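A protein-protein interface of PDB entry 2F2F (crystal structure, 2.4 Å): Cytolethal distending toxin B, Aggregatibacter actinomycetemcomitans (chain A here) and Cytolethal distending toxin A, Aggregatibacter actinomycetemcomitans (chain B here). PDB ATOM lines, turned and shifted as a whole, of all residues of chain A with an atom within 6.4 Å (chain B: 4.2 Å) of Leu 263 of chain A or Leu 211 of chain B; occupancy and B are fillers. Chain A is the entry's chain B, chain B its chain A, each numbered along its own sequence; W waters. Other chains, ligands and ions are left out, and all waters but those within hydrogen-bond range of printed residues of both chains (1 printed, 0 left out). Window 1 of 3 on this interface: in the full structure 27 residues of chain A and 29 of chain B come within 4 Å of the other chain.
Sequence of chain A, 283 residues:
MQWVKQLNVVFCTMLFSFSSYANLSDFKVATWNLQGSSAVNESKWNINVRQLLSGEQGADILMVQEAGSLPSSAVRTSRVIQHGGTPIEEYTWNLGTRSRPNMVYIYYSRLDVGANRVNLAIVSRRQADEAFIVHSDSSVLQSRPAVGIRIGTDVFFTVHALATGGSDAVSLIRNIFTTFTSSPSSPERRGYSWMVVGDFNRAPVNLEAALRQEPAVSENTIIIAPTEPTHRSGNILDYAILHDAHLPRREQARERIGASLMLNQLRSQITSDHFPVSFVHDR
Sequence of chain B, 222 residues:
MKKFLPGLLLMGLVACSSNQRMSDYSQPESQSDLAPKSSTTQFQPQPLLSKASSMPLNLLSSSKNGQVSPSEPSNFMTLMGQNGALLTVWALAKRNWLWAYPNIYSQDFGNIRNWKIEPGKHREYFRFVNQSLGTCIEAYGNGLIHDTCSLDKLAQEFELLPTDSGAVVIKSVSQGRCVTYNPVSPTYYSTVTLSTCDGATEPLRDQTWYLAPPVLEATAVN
Among the printed residues, pairs that only touch across the chains: Leu 263 of chain A with Leu 160 of chain B (3.4 Å), Leu 263 of chain A with Leu 211 of chain B (3.2 Å), Leu 266 of chain A with Leu 211 of chain B (3.5 Å), Arg 267 of chain A with Met 77 of chain B (3.7 Å), Arg 267 of chain A with Leu 211 of chain B (3.2 Å), Arg 267 of chain A with Ala 212 of chain B (3.8 Å) and Ser 268 of chain A with Leu 211 of chain B (3.5 Å).
The backbone carbonyl oxygen of Ala 212 of chain B lies within hydrogen-bond range of the backbone NH of Thr 78 of chain B. NH1 of Arg 267 of chain A sits at hydrogen-bond distance from O of Asn 264 of chain A, 3.2 Å away.
Of the 8 printed residues of chain B, 4 touch a printed residue of chain A. Along chain B the printed residues that touch a printed residue of chain A span positions 77 to 212. Of the 13 printed residues of chain A, 4 touch a printed residue of chain B. Hydrophobic or aromatic side chains of chain A within 4 Å of the printed part of chain B: Leu 263.
Water W1 bridges O of Leu 211 of chain B (2.9 Å) and O of Ser 268 of chain A (3.3 Å).
Printed residues of chain B within 4 Å of Leu 263 of chain A: Leu 160 (3.4 Å) and Leu 211 (3.2 Å). Printed residues of chain B within 4 Å of Leu 266 of chain A: Leu 211. Printed residues of chain B within 4 Å of Ser 268 of chain A: Leu 211 (3.5 Å). Of the printed residues of chain A, Met 77 of chain B touches Arg 267 (3.7 Å). Of chain A, only Leu 263 (3.2 Å), Leu 266 (3.5 Å), Arg 267 (3.2 Å) and Ser 268 (3.5 Å) come within 4 Å of Leu 211 of chain B. The nearest printed residue of chain A that does not touch Ala 212 of chain B is Leu 266 of chain A (4.6 Å).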
ATOM      1  N   SER A 260      -5.321  20.393  -4.236  1.00  0.00           N
ATOM      2  CA  SER A 260      -4.630  19.194  -4.682  1.00  0.00           C
ATOM      3  C   SER A 260      -4.049  18.446  -3.496  1.00  0.00           C
ATOM      4  O   SER A 260      -3.864  19.025  -2.437  1.00  0.00           O
ATOM      5  CB  SER A 260      -3.512  19.560  -5.660  1.00  0.00           C
ATOM      6  OG  SER A 260      -2.319  19.885  -4.974  1.00  0.00           O
ATOM      7  N   LEU A 261      -3.783  17.157  -3.666  1.00  0.00           N
ATOM      8  CA  LEU A 261      -3.174  16.388  -2.586  1.00  0.00           C
ATOM      9  C   LEU A 261      -1.809  17.031  -2.322  1.00  0.00           C
ATOM     10  O   LEU A 261      -1.128  17.455  -3.257  1.00  0.00           O
ATOM     11  CB  LEU A 261      -3.022  14.924  -2.996  1.00  0.00           C
ATOM     12  CG  LEU A 261      -4.326  14.167  -3.228  1.00  0.00           C
ATOM     13  CD1 LEU A 261      -4.014  12.691  -3.458  1.00  0.00           C
ATOM     14  CD2 LEU A 261      -5.253  14.331  -2.015  1.00  0.00           C
ATOM     15  N   MET A 262      -1.430  17.104  -1.052  1.00  0.00           N
ATOM     16  CA  MET A 262      -0.196  17.727  -0.612  1.00  0.00           C
ATOM     17  C   MET A 262       0.933  16.697  -0.413  1.00  0.00           C
ATOM     18  O   MET A 262       1.719  16.768   0.544  1.00  0.00           O
ATOM     19  CB  MET A 262      -0.476  18.465   0.692  1.00  0.00           C
ATOM     20  CG  MET A 262       0.196  19.784   0.821  1.00  0.00           C
ATOM     21  SD  MET A 262       0.051  20.371   2.497  1.00  0.00           S
ATOM     22  CE  MET A 262       1.079  21.839   2.449  1.00  0.00           C
ATOM     23  N   LEU A 263       0.990  15.714  -1.303  1.00  0.00           N
ATOM     24  CA  LEU A 263       2.013  14.686  -1.205  1.00  0.00           C
ATOM     25  C   LEU A 263       3.422  15.219  -1.424  1.00  0.00           C
ATOM     26  O   LEU A 263       4.388  14.564  -1.072  1.00  0.00           O
ATOM     27  CB  LEU A 263       1.713  13.563  -2.192  1.00  0.00           C
ATOM     28  CG  LEU A 263       0.285  13.004  -2.185  1.00  0.00           C
ATOM     29  CD1 LEU A 263       0.164  11.980  -3.283  1.00  0.00           C
ATOM     30  CD2 LEU A 263      -0.059  12.380  -0.850  1.00  0.00           C
ATOM     31  N   ASN A 264       3.536  16.429  -1.959  1.00  0.00           N
ATOM     32  CA  ASN A 264       4.846  17.033  -2.201  1.00  0.00           C
ATOM     33  C   ASN A 264       5.525  17.403  -0.907  1.00  0.00           C
ATOM     34  O   ASN A 264       6.705  17.768  -0.898  1.00  0.00           O
ATOM     35  CB  ASN A 264       4.706  18.283  -3.071  1.00  0.00           C
ATOM     36  CG  ASN A 264       3.831  19.353  -2.429  1.00  0.00           C
ATOM     37  OD1 ASN A 264       2.617  19.203  -2.348  1.00  0.00           O
ATOM     38  ND2 ASN A 264       4.451  20.431  -1.969  1.00  0.00           N
ATOM     39  N   GLN A 265       4.778  17.334   0.190  1.00  0.00           N
ATOM     40  CA  GLN A 265       5.305  17.688   1.511  1.00  0.00           C
ATOM     41  C   GLN A 265       5.770  16.481   2.335  1.00  0.00           C
ATOM     42  O   GLN A 265       6.418  16.643   3.368  1.00  0.00           O
ATOM     43  CB  GLN A 265       4.225  18.423   2.316  1.00  0.00           C
ATOM     44  CG  GLN A 265       3.958  19.856   1.906  1.00  0.00           C
ATOM     45  CD  GLN A 265       5.148  20.743   2.109  1.00  0.00           C
ATOM     46  OE1 GLN A 265       5.849  21.067   1.159  1.00  0.00           O
ATOM     47  NE2 GLN A 265       5.388  21.145   3.351  1.00  0.00           N
ATOM     48  N   LEU A 266       5.427  15.277   1.900  1.00  0.00           N
ATOM     49  CA  LEU A 266       5.790  14.090   2.665  1.00  0.00           C
ATOM     50  C   LEU A 266       7.190  13.499   2.494  1.00  0.00           C
ATOM     51  O   LEU A 266       7.743  13.460   1.402  1.00  0.00           O
ATOM     52  CB  LEU A 266       4.761  12.985   2.406  1.00  0.00           C
ATOM     53  CG  LEU A 266       3.290  13.394   2.330  1.00  0.00           C
ATOM     54  CD1 LEU A 266       2.473  12.204   1.906  1.00  0.00           C
ATOM     55  CD2 LEU A 266       2.800  13.922   3.661  1.00  0.00           C
ATOM     56  N   ARG A 267       7.724  13.022   3.612  1.00  0.00           N
ATOM     57  CA  ARG A 267       9.017  12.359   3.704  1.00  0.00           C
ATOM     58  C   ARG A 267       8.812  11.018   4.444  1.00  0.00           C
ATOM     59  O   ARG A 267       9.770  10.360   4.852  1.00  0.00           O
ATOM     60  CB  ARG A 267       9.998  13.229   4.479  1.00  0.00           C
ATOM     61  CG  ARG A 267       9.975  14.679   4.071  1.00  0.00           C
ATOM     62  CD  ARG A 267      10.454  14.895   2.651  1.00  0.00           C
ATOM     63  NE  ARG A 267      10.619  16.316   2.349  1.00  0.00           N
ATOM     64  CZ  ARG A 267       9.969  16.958   1.379  1.00  0.00           C
ATOM     65  NH1 ARG A 267       9.100  16.318   0.605  1.00  0.00           N
ATOM     66  NH2 ARG A 267      10.195  18.247   1.169  1.00  0.00           N
ATOM     67  N   SER A 268       7.549  10.684   4.689  1.00  0.00           N
ATOM     68  CA  SER A 268       7.185   9.465   5.395  1.00  0.00           C
ATOM     69  C   SER A 268       5.856   8.918   4.960  1.00  0.00           C
ATOM     70  O   SER A 268       5.153   9.500   4.141  1.00  0.00           O
ATOM     71  CB  SER A 268       7.050   9.691   6.902  1.00  0.00           C
ATOM     72  OG  SER A 268       7.866  10.740   7.375  1.00  0.00           O
ATOM     73  N   GLN A 269       5.525   7.776   5.543  1.00  0.00           N
ATOM     74  CA  GLN A 269       4.260   7.128   5.294  1.00  0.00           C
ATOM     75  C   GLN A 269       3.201   8.097   5.833  1.00  0.00           C
ATOM     76  O   GLN A 269       3.450   8.787   6.816  1.00  0.00           O
ATOM     77  CB  GLN A 269       4.215   5.823   6.098  1.00  0.00           C
ATOM     78  CG  GLN A 269       2.859   5.229   6.327  1.00  0.00           C
ATOM     79  CD  GLN A 269       2.256   4.796   5.044  1.00  0.00           C
ATOM     80  OE1 GLN A 269       2.262   5.550   4.080  1.00  0.00           O
ATOM     81  NE2 GLN A 269       1.738   3.581   5.000  1.00  0.00           N
ATOM     82  N   ILE A 270       2.029   8.155   5.205  1.00  0.00           N
ATOM     83  CA  ILE A 270       0.951   9.007   5.720  1.00  0.00           C
ATOM     84  C   ILE A 270       0.336   8.151   6.804  1.00  0.00           C
ATOM     85  O   ILE A 270      -0.190   7.089   6.505  1.00  0.00           O
ATOM     86  CB  ILE A 270      -0.156   9.282   4.695  1.00  0.00           C
ATOM     87  CG1 ILE A 270       0.462   9.640   3.344  1.00  0.00           C
ATOM     88  CG2 ILE A 270      -1.038  10.432   5.190  1.00  0.00           C
ATOM     89  CD1 ILE A 270       0.772   8.421   2.469  1.00  0.00           C
ATOM     90  N   PHE A 275      -5.557  11.578   3.031  1.00  0.00           N
ATOM     91  CA  PHE A 275      -4.394  12.246   2.443  1.00  0.00           C
ATOM     92  C   PHE A 275      -4.496  13.757   2.678  1.00  0.00           C
ATOM     93  O   PHE A 275      -5.590  14.328   2.624  1.00  0.00           O
ATOM     94  CB  PHE A 275      -4.338  11.925   0.945  1.00  0.00           C
ATOM     95  CG  PHE A 275      -4.305  10.445   0.656  1.00  0.00           C
ATOM     96  CD1 PHE A 275      -3.294   9.651   1.193  1.00  0.00           C
ATOM     97  CD2 PHE A 275      -5.314   9.827  -0.070  1.00  0.00           C
ATOM     98  CE1 PHE A 275      -3.299   8.277   1.015  1.00  0.00           C
ATOM     99  CE2 PHE A 275      -5.329   8.447  -0.254  1.00  0.00           C
ATOM    100  CZ  PHE A 275      -4.320   7.673   0.291  1.00  0.00           C
ATOM    101  N   PRO A 276      -3.362  14.416   2.971  1.00  0.00           N
ATOM    102  CA  PRO A 276      -3.399  15.865   3.206  1.00  0.00           C
ATOM    103  C   PRO A 276      -3.745  16.594   1.898  1.00  0.00           C
ATOM    104  O   PRO A 276      -3.302  16.195   0.823  1.00  0.00           O
ATOM    105  CB  PRO A 276      -1.995  16.193   3.719  1.00  0.00           C
ATOM    106  CG  PRO A 276      -1.127  15.028   3.294  1.00  0.00           C
ATOM    107  CD  PRO A 276      -2.003  13.844   3.107  1.00  0.00           C
ATOM    108  N   MET B  77      13.899  16.008  -1.119  1.00  0.00           N
ATOM    109  CA  MET B  77      13.548  14.639  -0.791  1.00  0.00           C
ATOM    110  C   MET B  77      14.124  13.682  -1.827  1.00  0.00           C
ATOM    111  O   MET B  77      14.801  14.097  -2.757  1.00  0.00           O
ATOM    112  CB  MET B  77      12.029  14.474  -0.794  1.00  0.00           C
ATOM    113  CG  MET B  77      11.362  15.016  -2.032  1.00  0.00           C
ATOM    114  SD  MET B  77      11.326  13.909  -3.428  1.00  0.00           S
ATOM    115  CE  MET B  77       9.855  13.024  -3.143  1.00  0.00           C
ATOM    116  N   THR B  78      13.885  12.390  -1.637  1.00  0.00           N
ATOM    117  CA  THR B  78      14.343  11.405  -2.599  1.00  0.00           C
ATOM    118  C   THR B  78      13.143  10.577  -2.980  1.00  0.00           C
ATOM    119  O   THR B  78      12.252  10.403  -2.165  1.00  0.00           O
ATOM    120  CB  THR B  78      15.417  10.478  -2.010  1.00  0.00           C
ATOM    121  OG1 THR B  78      14.977   9.970  -0.743  1.00  0.00           O
ATOM    122  CG2 THR B  78      16.737  11.231  -1.847  1.00  0.00           C
ATOM    123  N   LEU B  79      13.107  10.094  -4.217  1.00  0.00           N
ATOM    124  CA  LEU B  79      12.038   9.228  -4.668  1.00  0.00           C
ATOM    125  C   LEU B  79      12.689   7.833  -4.611  1.00  0.00           C
ATOM    126  O   LEU B  79      13.459   7.467  -5.496  1.00  0.00           O
ATOM    127  CB  LEU B  79      11.646   9.587  -6.097  1.00  0.00           C
ATOM    128  CG  LEU B  79      10.669  10.752  -6.201  1.00  0.00           C
ATOM    129  CD1 LEU B  79      10.757  11.367  -7.599  1.00  0.00           C
ATOM    130  CD2 LEU B  79       9.245  10.253  -5.898  1.00  0.00           C
ATOM    131  N   LEU B 160       1.139  12.523  -8.972  1.00  0.00           N
ATOM    132  CA  LEU B 160       1.603  11.660  -7.905  1.00  0.00           C
ATOM    133  C   LEU B 160       0.325  10.972  -7.421  1.00  0.00           C
ATOM    134  O   LEU B 160      -0.409  11.515  -6.604  1.00  0.00           O
ATOM    135  CB  LEU B 160       2.227  12.501  -6.790  1.00  0.00           C
ATOM    136  CG  LEU B 160       3.634  13.056  -7.011  1.00  0.00           C
ATOM    137  CD1 LEU B 160       4.080  13.790  -5.768  1.00  0.00           C
ATOM    138  CD2 LEU B 160       4.606  11.922  -7.332  1.00  0.00           C
ATOM    139  N   VAL B 168       3.499   5.823  -3.854  1.00  0.00           N
ATOM    140  CA  VAL B 168       2.910   6.551  -4.962  1.00  0.00           C
ATOM    141  C   VAL B 168       3.370   5.958  -6.276  1.00  0.00           C
ATOM    142  O   VAL B 168       4.360   5.235  -6.338  1.00  0.00           O
ATOM    143  CB  VAL B 168       3.284   8.070  -4.924  1.00  0.00           C
ATOM    144  CG1 VAL B 168       2.552   8.746  -3.793  1.00  0.00           C
ATOM    145  CG2 VAL B 168       4.788   8.252  -4.737  1.00  0.00           C
ATOM    146  N   TYR B 210       8.525   5.672  -2.916  1.00  0.00           N
ATOM    147  CA  TYR B 210       8.237   6.221  -1.614  1.00  0.00           C
ATOM    148  C   TYR B 210       8.754   7.652  -1.627  1.00  0.00           C
ATOM    149  O   TYR B 210       9.817   7.925  -2.184  1.00  0.00           O
ATOM    150  CB  TYR B 210       8.960   5.423  -0.512  1.00  0.00           C
ATOM    151  CG  TYR B 210       8.839   3.904  -0.610  1.00  0.00           C
ATOM    152  CD1 TYR B 210       7.635   3.290  -0.967  1.00  0.00           C
ATOM    153  CD2 TYR B 210       9.936   3.080  -0.321  1.00  0.00           C
ATOM    154  CE1 TYR B 210       7.525   1.897  -1.033  1.00  0.00           C
ATOM    155  CE2 TYR B 210       9.837   1.687  -0.384  1.00  0.00           C
ATOM    156  CZ  TYR B 210       8.630   1.102  -0.739  1.00  0.00           C
ATOM    157  OH  TYR B 210       8.525  -0.269  -0.774  1.00  0.00           O
ATOM    158  N   LEU B 211       7.976   8.565  -1.056  1.00  0.00           N
ATOM    159  CA  LEU B 211       8.375   9.958  -0.942  1.00  0.00           C
ATOM    160  C   LEU B 211       9.153   9.907   0.360  1.00  0.00           C
ATOM    161  O   LEU B 211       8.566   9.851   1.431  1.00  0.00           O
ATOM    162  CB  LEU B 211       7.146  10.853  -0.809  1.00  0.00           C
ATOM    163  CG  LEU B 211       6.143  10.681  -1.946  1.00  0.00           C
ATOM    164  CD1 LEU B 211       4.873  11.439  -1.622  1.00  0.00           C
ATOM    165  CD2 LEU B 211       6.735  11.188  -3.257  1.00  0.00           C
ATOM    166  N   ALA B 212      10.475   9.941   0.267  1.00  0.00           N
ATOM    167  CA  ALA B 212      11.315   9.814   1.457  1.00  0.00           C
ATOM    168  C   ALA B 212      12.240  10.985   1.689  1.00  0.00           C
ATOM    169  O   ALA B 212      12.344  11.884   0.855  1.00  0.00           O
ATOM    170  CB  ALA B 212      12.145   8.529   1.356  1.00  0.00           C
HETATM  171  O   HOH W   1       6.635   7.780   1.782  1.00  0.00           O
